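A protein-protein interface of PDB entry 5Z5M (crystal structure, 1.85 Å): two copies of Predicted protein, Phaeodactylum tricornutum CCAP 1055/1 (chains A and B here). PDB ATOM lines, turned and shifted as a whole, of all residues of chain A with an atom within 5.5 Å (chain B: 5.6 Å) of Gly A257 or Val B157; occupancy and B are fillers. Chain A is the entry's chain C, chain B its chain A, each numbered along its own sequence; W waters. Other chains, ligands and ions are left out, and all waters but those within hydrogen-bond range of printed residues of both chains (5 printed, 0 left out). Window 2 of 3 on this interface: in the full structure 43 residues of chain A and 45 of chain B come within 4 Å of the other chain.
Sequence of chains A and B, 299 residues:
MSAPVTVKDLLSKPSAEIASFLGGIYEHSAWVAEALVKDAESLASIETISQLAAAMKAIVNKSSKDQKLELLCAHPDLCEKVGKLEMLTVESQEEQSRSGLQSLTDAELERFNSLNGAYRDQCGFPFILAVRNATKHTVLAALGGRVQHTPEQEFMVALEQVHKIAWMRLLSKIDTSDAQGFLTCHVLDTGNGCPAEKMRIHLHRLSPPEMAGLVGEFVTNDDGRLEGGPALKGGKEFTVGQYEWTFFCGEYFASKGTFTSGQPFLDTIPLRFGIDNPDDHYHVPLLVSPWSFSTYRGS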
ATOM      1  N   PHE A 253      24.610  -0.390  30.849  1.00  0.00           N
ATOM      2  CA  PHE A 253      23.876   0.580  30.034  1.00  0.00           C
ATOM      3  C   PHE A 253      24.488   0.673  28.639  1.00  0.00           C
ATOM      4  O   PHE A 253      23.774   0.826  27.647  1.00  0.00           O
ATOM      5  CB  PHE A 253      23.831   1.963  30.715  1.00  0.00           C
ATOM      6  CG  PHE A 253      22.974   1.992  31.954  1.00  0.00           C
ATOM      7  CD1 PHE A 253      21.639   1.618  31.889  1.00  0.00           C
ATOM      8  CD2 PHE A 253      23.498   2.382  33.180  1.00  0.00           C
ATOM      9  CE1 PHE A 253      20.845   1.620  33.021  1.00  0.00           C
ATOM     10  CE2 PHE A 253      22.705   2.398  34.318  1.00  0.00           C
ATOM     11  CZ  PHE A 253      21.378   2.013  34.240  1.00  0.00           C
ATOM     12  N   ALA A 254      25.807   0.548  28.553  1.00  0.00           N
ATOM     13  CA  ALA A 254      26.473   0.531  27.255  1.00  0.00           C
ATOM     14  C   ALA A 254      25.972  -0.622  26.384  1.00  0.00           C
ATOM     15  O   ALA A 254      25.805  -0.464  25.178  1.00  0.00           O
ATOM     16  CB  ALA A 254      27.988   0.443  27.435  1.00  0.00           C
ATOM     17  N   SER A 255      25.718  -1.775  27.002  1.00  0.00           N
ATOM     18  CA  SER A 255      25.289  -2.959  26.263  1.00  0.00           C
ATOM     19  C   SER A 255      23.899  -2.781  25.654  1.00  0.00           C
ATOM     20  O   SER A 255      23.552  -3.443  24.675  1.00  0.00           O
ATOM     21  CB  SER A 255      25.312  -4.200  27.166  1.00  0.00           C
ATOM     22  OG  SER A 255      24.212  -4.232  28.062  1.00  0.00           O
ATOM     23  N   LYS A 256      23.107  -1.885  26.229  1.00  0.00           N
ATOM     24  CA  LYS A 256      21.760  -1.634  25.732  1.00  0.00           C
ATOM     25  C   LYS A 256      21.725  -0.409  24.825  1.00  0.00           C
ATOM     26  O   LYS A 256      20.682  -0.068  24.275  1.00  0.00           O
ATOM     27  CB  LYS A 256      20.784  -1.448  26.899  1.00  0.00           C
ATOM     28  CG  LYS A 256      20.728  -2.630  27.851  1.00  0.00           C
ATOM     29  CD  LYS A 256      19.306  -2.910  28.295  1.00  0.00           C
ATOM     30  CE  LYS A 256      19.189  -4.294  28.900  1.00  0.00           C
ATOM     31  NZ  LYS A 256      17.802  -4.577  29.356  1.00  0.00           N
ATOM     32  N   GLY A 257      22.866   0.255  24.683  1.00  0.00           N
ATOM     33  CA  GLY A 257      22.936   1.497  23.934  1.00  0.00           C
ATOM     34  C   GLY A 257      22.143   2.618  24.587  1.00  0.00           C
ATOM     35  O   GLY A 257      21.755   3.575  23.923  1.00  0.00           O
ATOM     36  N   THR A 258      21.898   2.488  25.889  1.00  0.00           N
ATOM     37  CA  THR A 258      21.176   3.501  26.655  1.00  0.00           C
ATOM     38  C   THR A 258      21.969   4.794  26.666  1.00  0.00           C
ATOM     39  O   THR A 258      23.186   4.773  26.860  1.00  0.00           O
ATOM     40  CB  THR A 258      20.932   3.046  28.111  1.00  0.00           C
ATOM     41  OG1 THR A 258      20.253   1.787  28.108  1.00  0.00           O
ATOM     42  CG2 THR A 258      20.096   4.081  28.875  1.00  0.00           C
ATOM     43  N   PHE A 259      21.296   5.918  26.453  1.00  0.00           N
ATOM     44  CA  PHE A 259      22.009   7.188  26.411  1.00  0.00           C
ATOM     45  C   PHE A 259      22.613   7.525  27.767  1.00  0.00           C
ATOM     46  O   PHE A 259      21.919   7.523  28.779  1.00  0.00           O
ATOM     47  CB  PHE A 259      21.106   8.334  25.968  1.00  0.00           C
ATOM     48  CG  PHE A 259      21.791   9.672  26.015  1.00  0.00           C
ATOM     49  CD1 PHE A 259      22.651  10.056  24.996  1.00  0.00           C
ATOM     50  CD2 PHE A 259      21.613  10.523  27.093  1.00  0.00           C
ATOM     51  CE1 PHE A 259      23.299  11.275  25.038  1.00  0.00           C
ATOM     52  CE2 PHE A 259      22.258  11.747  27.143  1.00  0.00           C
ATOM     53  CZ  PHE A 259      23.103  12.123  26.113  1.00  0.00           C
ATOM     54  N   ARG B 146      24.732  -4.393  21.338  1.00  0.00           N
ATOM     55  CA  ARG B 146      24.238  -3.587  20.227  1.00  0.00           C
ATOM     56  C   ARG B 146      24.238  -4.336  18.892  1.00  0.00           C
ATOM     57  O   ARG B 146      23.580  -3.923  17.939  1.00  0.00           O
ATOM     58  CB  ARG B 146      25.053  -2.292  20.132  1.00  0.00           C
ATOM     59  CG  ARG B 146      24.691  -1.290  21.236  1.00  0.00           C
ATOM     60  CD  ARG B 146      25.692  -0.148  21.366  1.00  0.00           C
ATOM     61  NE  ARG B 146      25.948   0.525  20.098  1.00  0.00           N
ATOM     62  CZ  ARG B 146      26.910   1.423  19.913  1.00  0.00           C
ATOM     63  NH1 ARG B 146      27.697   1.774  20.925  1.00  0.00           N
ATOM     64  NH2 ARG B 146      27.083   1.977  18.720  1.00  0.00           N
ATOM     65  N   HIS B 149      20.726  -5.357  18.016  1.00  0.00           N
ATOM     66  CA  HIS B 149      19.741  -4.326  17.700  1.00  0.00           C
ATOM     67  C   HIS B 149      19.487  -4.189  16.204  1.00  0.00           C
ATOM     68  O   HIS B 149      20.296  -4.615  15.383  1.00  0.00           O
ATOM     69  CB  HIS B 149      20.188  -2.972  18.260  1.00  0.00           C
ATOM     70  CG  HIS B 149      20.278  -2.934  19.751  1.00  0.00           C
ATOM     71  ND1 HIS B 149      20.837  -1.878  20.436  1.00  0.00           N
ATOM     72  CD2 HIS B 149      19.879  -3.825  20.692  1.00  0.00           C
ATOM     73  CE1 HIS B 149      20.779  -2.117  21.734  1.00  0.00           C
ATOM     74  NE2 HIS B 149      20.199  -3.292  21.915  1.00  0.00           N
ATOM     75  N   GLU B 152      18.036   0.602  12.483  1.00  0.00           N
ATOM     76  CA  GLU B 152      17.453   1.916  12.727  1.00  0.00           C
ATOM     77  C   GLU B 152      17.627   2.344  14.178  1.00  0.00           C
ATOM     78  O   GLU B 152      17.767   3.533  14.459  1.00  0.00           O
ATOM     79  CB  GLU B 152      15.968   1.954  12.344  1.00  0.00           C
ATOM     80  CG  GLU B 152      15.074   0.978  13.095  1.00  0.00           C
ATOM     81  CD  GLU B 152      14.966  -0.368  12.401  1.00  0.00           C
ATOM     82  OE1 GLU B 152      15.715  -0.603  11.426  1.00  0.00           O
ATOM     83  OE2 GLU B 152      14.122  -1.189  12.823  1.00  0.00           O
ATOM     84  N   GLN B 153      17.624   1.387  15.101  1.00  0.00           N
ATOM     85  CA  GLN B 153      17.929   1.717  16.485  1.00  0.00           C
ATOM     86  C   GLN B 153      19.397   2.107  16.590  1.00  0.00           C
ATOM     87  O   GLN B 153      19.738   3.088  17.245  1.00  0.00           O
ATOM     88  CB  GLN B 153      17.628   0.560  17.441  1.00  0.00           C
ATOM     89  CG  GLN B 153      17.933   0.932  18.896  1.00  0.00           C
ATOM     90  CD  GLN B 153      17.660  -0.186  19.882  1.00  0.00           C
ATOM     91  OE1 GLN B 153      17.057  -1.202  19.539  1.00  0.00           O
ATOM     92  NE2 GLN B 153      18.102   0.001  21.122  1.00  0.00           N
ATOM     93  N   GLU B 154      20.259   1.336  15.937  1.00  0.00           N
ATOM     94  CA  GLU B 154      21.693   1.584  16.012  1.00  0.00           C
ATOM     95  C   GLU B 154      22.112   2.866  15.306  1.00  0.00           C
ATOM     96  O   GLU B 154      23.126   3.464  15.661  1.00  0.00           O
ATOM     97  CB  GLU B 154      22.468   0.399  15.444  1.00  0.00           C
ATOM     98  CG  GLU B 154      22.674  -0.691  16.475  1.00  0.00           C
ATOM     99  CD  GLU B 154      23.220  -0.132  17.788  1.00  0.00           C
ATOM    100  OE1 GLU B 154      24.360   0.382  17.787  1.00  0.00           O
ATOM    101  OE2 GLU B 154      22.508  -0.192  18.811  1.00  0.00           O
ATOM    102  N   PHE B 155      21.340   3.282  14.306  1.00  0.00           N
ATOM    103  CA  PHE B 155      21.610   4.537  13.611  1.00  0.00           C
ATOM    104  C   PHE B 155      21.472   5.704  14.590  1.00  0.00           C
ATOM    105  O   PHE B 155      22.296   6.615  14.603  1.00  0.00           O
ATOM    106  CB  PHE B 155      20.667   4.706  12.417  1.00  0.00           C
ATOM    107  CG  PHE B 155      20.961   5.916  11.572  1.00  0.00           C
ATOM    108  CD1 PHE B 155      22.015   5.913  10.675  1.00  0.00           C
ATOM    109  CD2 PHE B 155      20.168   7.049  11.662  1.00  0.00           C
ATOM    110  CE1 PHE B 155      22.284   7.021   9.892  1.00  0.00           C
ATOM    111  CE2 PHE B 155      20.428   8.160  10.878  1.00  0.00           C
ATOM    112  CZ  PHE B 155      21.487   8.146   9.993  1.00  0.00           C
ATOM    113  N   MET B 156      20.429   5.653  15.413  1.00  0.00           N
ATOM    114  CA  MET B 156      20.222   6.625  16.487  1.00  0.00           C
ATOM    115  C   MET B 156      21.313   6.582  17.549  1.00  0.00           C
ATOM    116  O   MET B 156      21.799   7.616  18.000  1.00  0.00           O
ATOM    117  CB  MET B 156      18.867   6.391  17.153  1.00  0.00           C
ATOM    118  CG  MET B 156      17.706   6.892  16.346  1.00  0.00           C
ATOM    119  SD  MET B 156      17.882   8.670  16.129  1.00  0.00           S
ATOM    120  CE  MET B 156      17.949   9.206  17.838  1.00  0.00           C
ATOM    121  N   VAL B 157      21.675   5.376  17.969  1.00  0.00           N
ATOM    122  CA  VAL B 157      22.695   5.213  18.995  1.00  0.00           C
ATOM    123  C   VAL B 157      24.048   5.715  18.494  1.00  0.00           C
ATOM    124  O   VAL B 157      24.768   6.392  19.217  1.00  0.00           O
ATOM    125  CB  VAL B 157      22.824   3.739  19.439  1.00  0.00           C
ATOM    126  CG1 VAL B 157      23.964   3.576  20.433  1.00  0.00           C
ATOM    127  CG2 VAL B 157      21.508   3.243  20.034  1.00  0.00           C
ATOM    128  N   ALA B 158      24.381   5.387  17.250  1.00  0.00           N
ATOM    129  CA  ALA B 158      25.655   5.804  16.669  1.00  0.00           C
ATOM    130  C   ALA B 158      25.754   7.325  16.609  1.00  0.00           C
ATOM    131  O   ALA B 158      26.802   7.900  16.902  1.00  0.00           O
ATOM    132  CB  ALA B 158      25.825   5.206  15.279  1.00  0.00           C
ATOM    133  N   LEU B 159      24.662   7.967  16.218  1.00  0.00           N
ATOM    134  CA  LEU B 159      24.639   9.423  16.125  1.00  0.00           C
ATOM    135  C   LEU B 159      24.793  10.059  17.505  1.00  0.00           C
ATOM    136  O   LEU B 159      25.440  11.093  17.642  1.00  0.00           O
ATOM    137  CB  LEU B 159      23.350   9.905  15.458  1.00  0.00           C
ATOM    138  CG  LEU B 159      23.230   9.677  13.948  1.00  0.00           C
ATOM    139  CD1 LEU B 159      21.832  10.031  13.467  1.00  0.00           C
ATOM    140  CD2 LEU B 159      24.278  10.474  13.184  1.00  0.00           C
ATOM    141  N   GLU B 160      24.208   9.439  18.524  1.00  0.00           N
ATOM    142  CA  GLU B 160      24.404   9.906  19.897  1.00  0.00           C
ATOM    143  C   GLU B 160      25.879   9.799  20.274  1.00  0.00           C
ATOM    144  O   GLU B 160      26.433  10.703  20.896  1.00  0.00           O
ATOM    145  CB  GLU B 160      23.531   9.113  20.876  1.00  0.00           C
ATOM    146  CG  GLU B 160      22.049   9.467  20.793  1.00  0.00           C
ATOM    147  CD  GLU B 160      21.156   8.582  21.652  1.00  0.00           C
ATOM    148  OE1 GLU B 160      21.653   7.592  22.241  1.00  0.00           O
ATOM    149  OE2 GLU B 160      19.947   8.889  21.738  1.00  0.00           O
ATOM    150  N   GLN B 161      26.517   8.698  19.876  1.00  0.00           N
ATOM    151  CA  GLN B 161      27.935   8.499  20.155  1.00  0.00           C
ATOM    152  C   GLN B 161      28.822   9.543  19.462  1.00  0.00           C
ATOM    153  O   GLN B 161      29.776  10.029  20.066  1.00  0.00           O
ATOM    154  CB  GLN B 161      28.376   7.084  19.753  1.00  0.00           C
ATOM    155  CG  GLN B 161      27.630   5.945  20.474  1.00  0.00           C
ATOM    156  CD  GLN B 161      27.830   5.931  21.988  1.00  0.00           C
ATOM    157  OE1 GLN B 161      28.943   6.095  22.489  1.00  0.00           O
ATOM    158  NE2 GLN B 161      26.744   5.730  22.721  1.00  0.00           N
ATOM    159  N   VAL B 162      28.523   9.911  18.213  1.00  0.00           N
ATOM    160  CA  VAL B 162      29.390  10.877  17.539  1.00  0.00           C
ATOM    161  C   VAL B 162      29.263  12.269  18.169  1.00  0.00           C
ATOM    162  O   VAL B 162      30.238  13.011  18.218  1.00  0.00           O
ATOM    163  CB  VAL B 162      29.124  10.975  16.007  1.00  0.00           C
ATOM    164  CG1 VAL B 162      29.300   9.615  15.343  1.00  0.00           C
ATOM    165  CG2 VAL B 162      27.761  11.555  15.709  1.00  0.00           C
HETATM  166  O   HOH W   1      20.085   5.393  23.040  1.00  0.00           O
HETATM  167  O   HOH W   2      26.955   1.712  23.799  1.00  0.00           O
HETATM  168  O   HOH W   3      23.612   6.080  23.155  1.00  0.00           O
HETATM  169  O   HOH W   4      25.166   6.617  25.063  1.00  0.00           O
HETATM  170  O   HOH W   5      17.864  -1.440  23.965  1.00  0.00           O
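Of the 7 printed residues of chain A, 5 touch a printed residue of chain B. Hydrophobic or aromatic side chains of chain A that line the printed part of chain B: Phe A259. Along chain A the printed residues that touch a printed residue of chain B span positions 254 to 259. Hydrophobic or aromatic side chains of chain B that line the printed part of chain A: His B149 and Val B157.
Water W1 lies within hydrogen-bond range of the backbone carbonyl oxygen of Gly A257 (2.6 Å) and the side-chain carboxylate of Glu B160 (2.8 Å). Water W3 lies within hydrogen-bond range of the side-chain carboxylate of Glu B160 (2.6 Å), the side-chain amide nitrogen of Gln B161 (3.2 Å) and the backbone carbonyl oxygen of Gly A257 (3.2 Å). Water W2 lies within hydrogen-bond range of the backbone carbonyl oxygen of Ala A254 (2.8 Å) and the guanidinium group of Arg B146 (3.0 Å). Water W4 lies within hydrogen-bond range of NE2 of Gln B161 (3.0 Å) and O of Thr A258 (3.2 Å). Water W5 lies within hydrogen-bond range of O of Lys A256 (3.1 Å) and NE2 of Gln B153 (3.2 Å).
Arg B146 touches Ala A254 (CD to O, 3.8 Å). O of Ser A255 touches N of Arg B146, at 3.7 Å. CE1 of His B149 touches O of Lys A256 (3.3 Å). Val B157 touches Gly A257 (CG2 to O, 3.9 Å). CD1 of Phe A259 touches OE1 of Glu B160 (3.8 Å).
NE of Arg B146 lies within salt-bridge range of OE1 of Glu B154 (2.8 Å). The side-chain amide nitrogen of Gln B153 lies within hydrogen-bond range of a ring nitrogen (ND1) of His B149. A ring nitrogen (ND1) of His B149 sits at hydrogen-bond distance from the side-chain carboxylate (OE2) of Glu B154 (2.9 Å).
Printed residues of chain B within 4 Å of Ala A254: Arg B146 (3.8 Å). Of the printed residues of chain B, Ser A255 touches Arg B146 (3.7 Å). Gly A257 touches just one residue of chain B: Val B157 (3.9 Å). Of the printed residues of chain A, Arg B146 touches Ala A254 and Ser A255. Printed residues of chain A within 4 Å of His B149: Lys A256. Phe B155 touches none of the printed residues of chain A. Val B157 touches just one residue of chain A: Gly A257 (3.9 Å). The nearest residue of chain A that does not touch Val B157 is Lys A256 (5.4 Å).
No position is printed for both chains.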
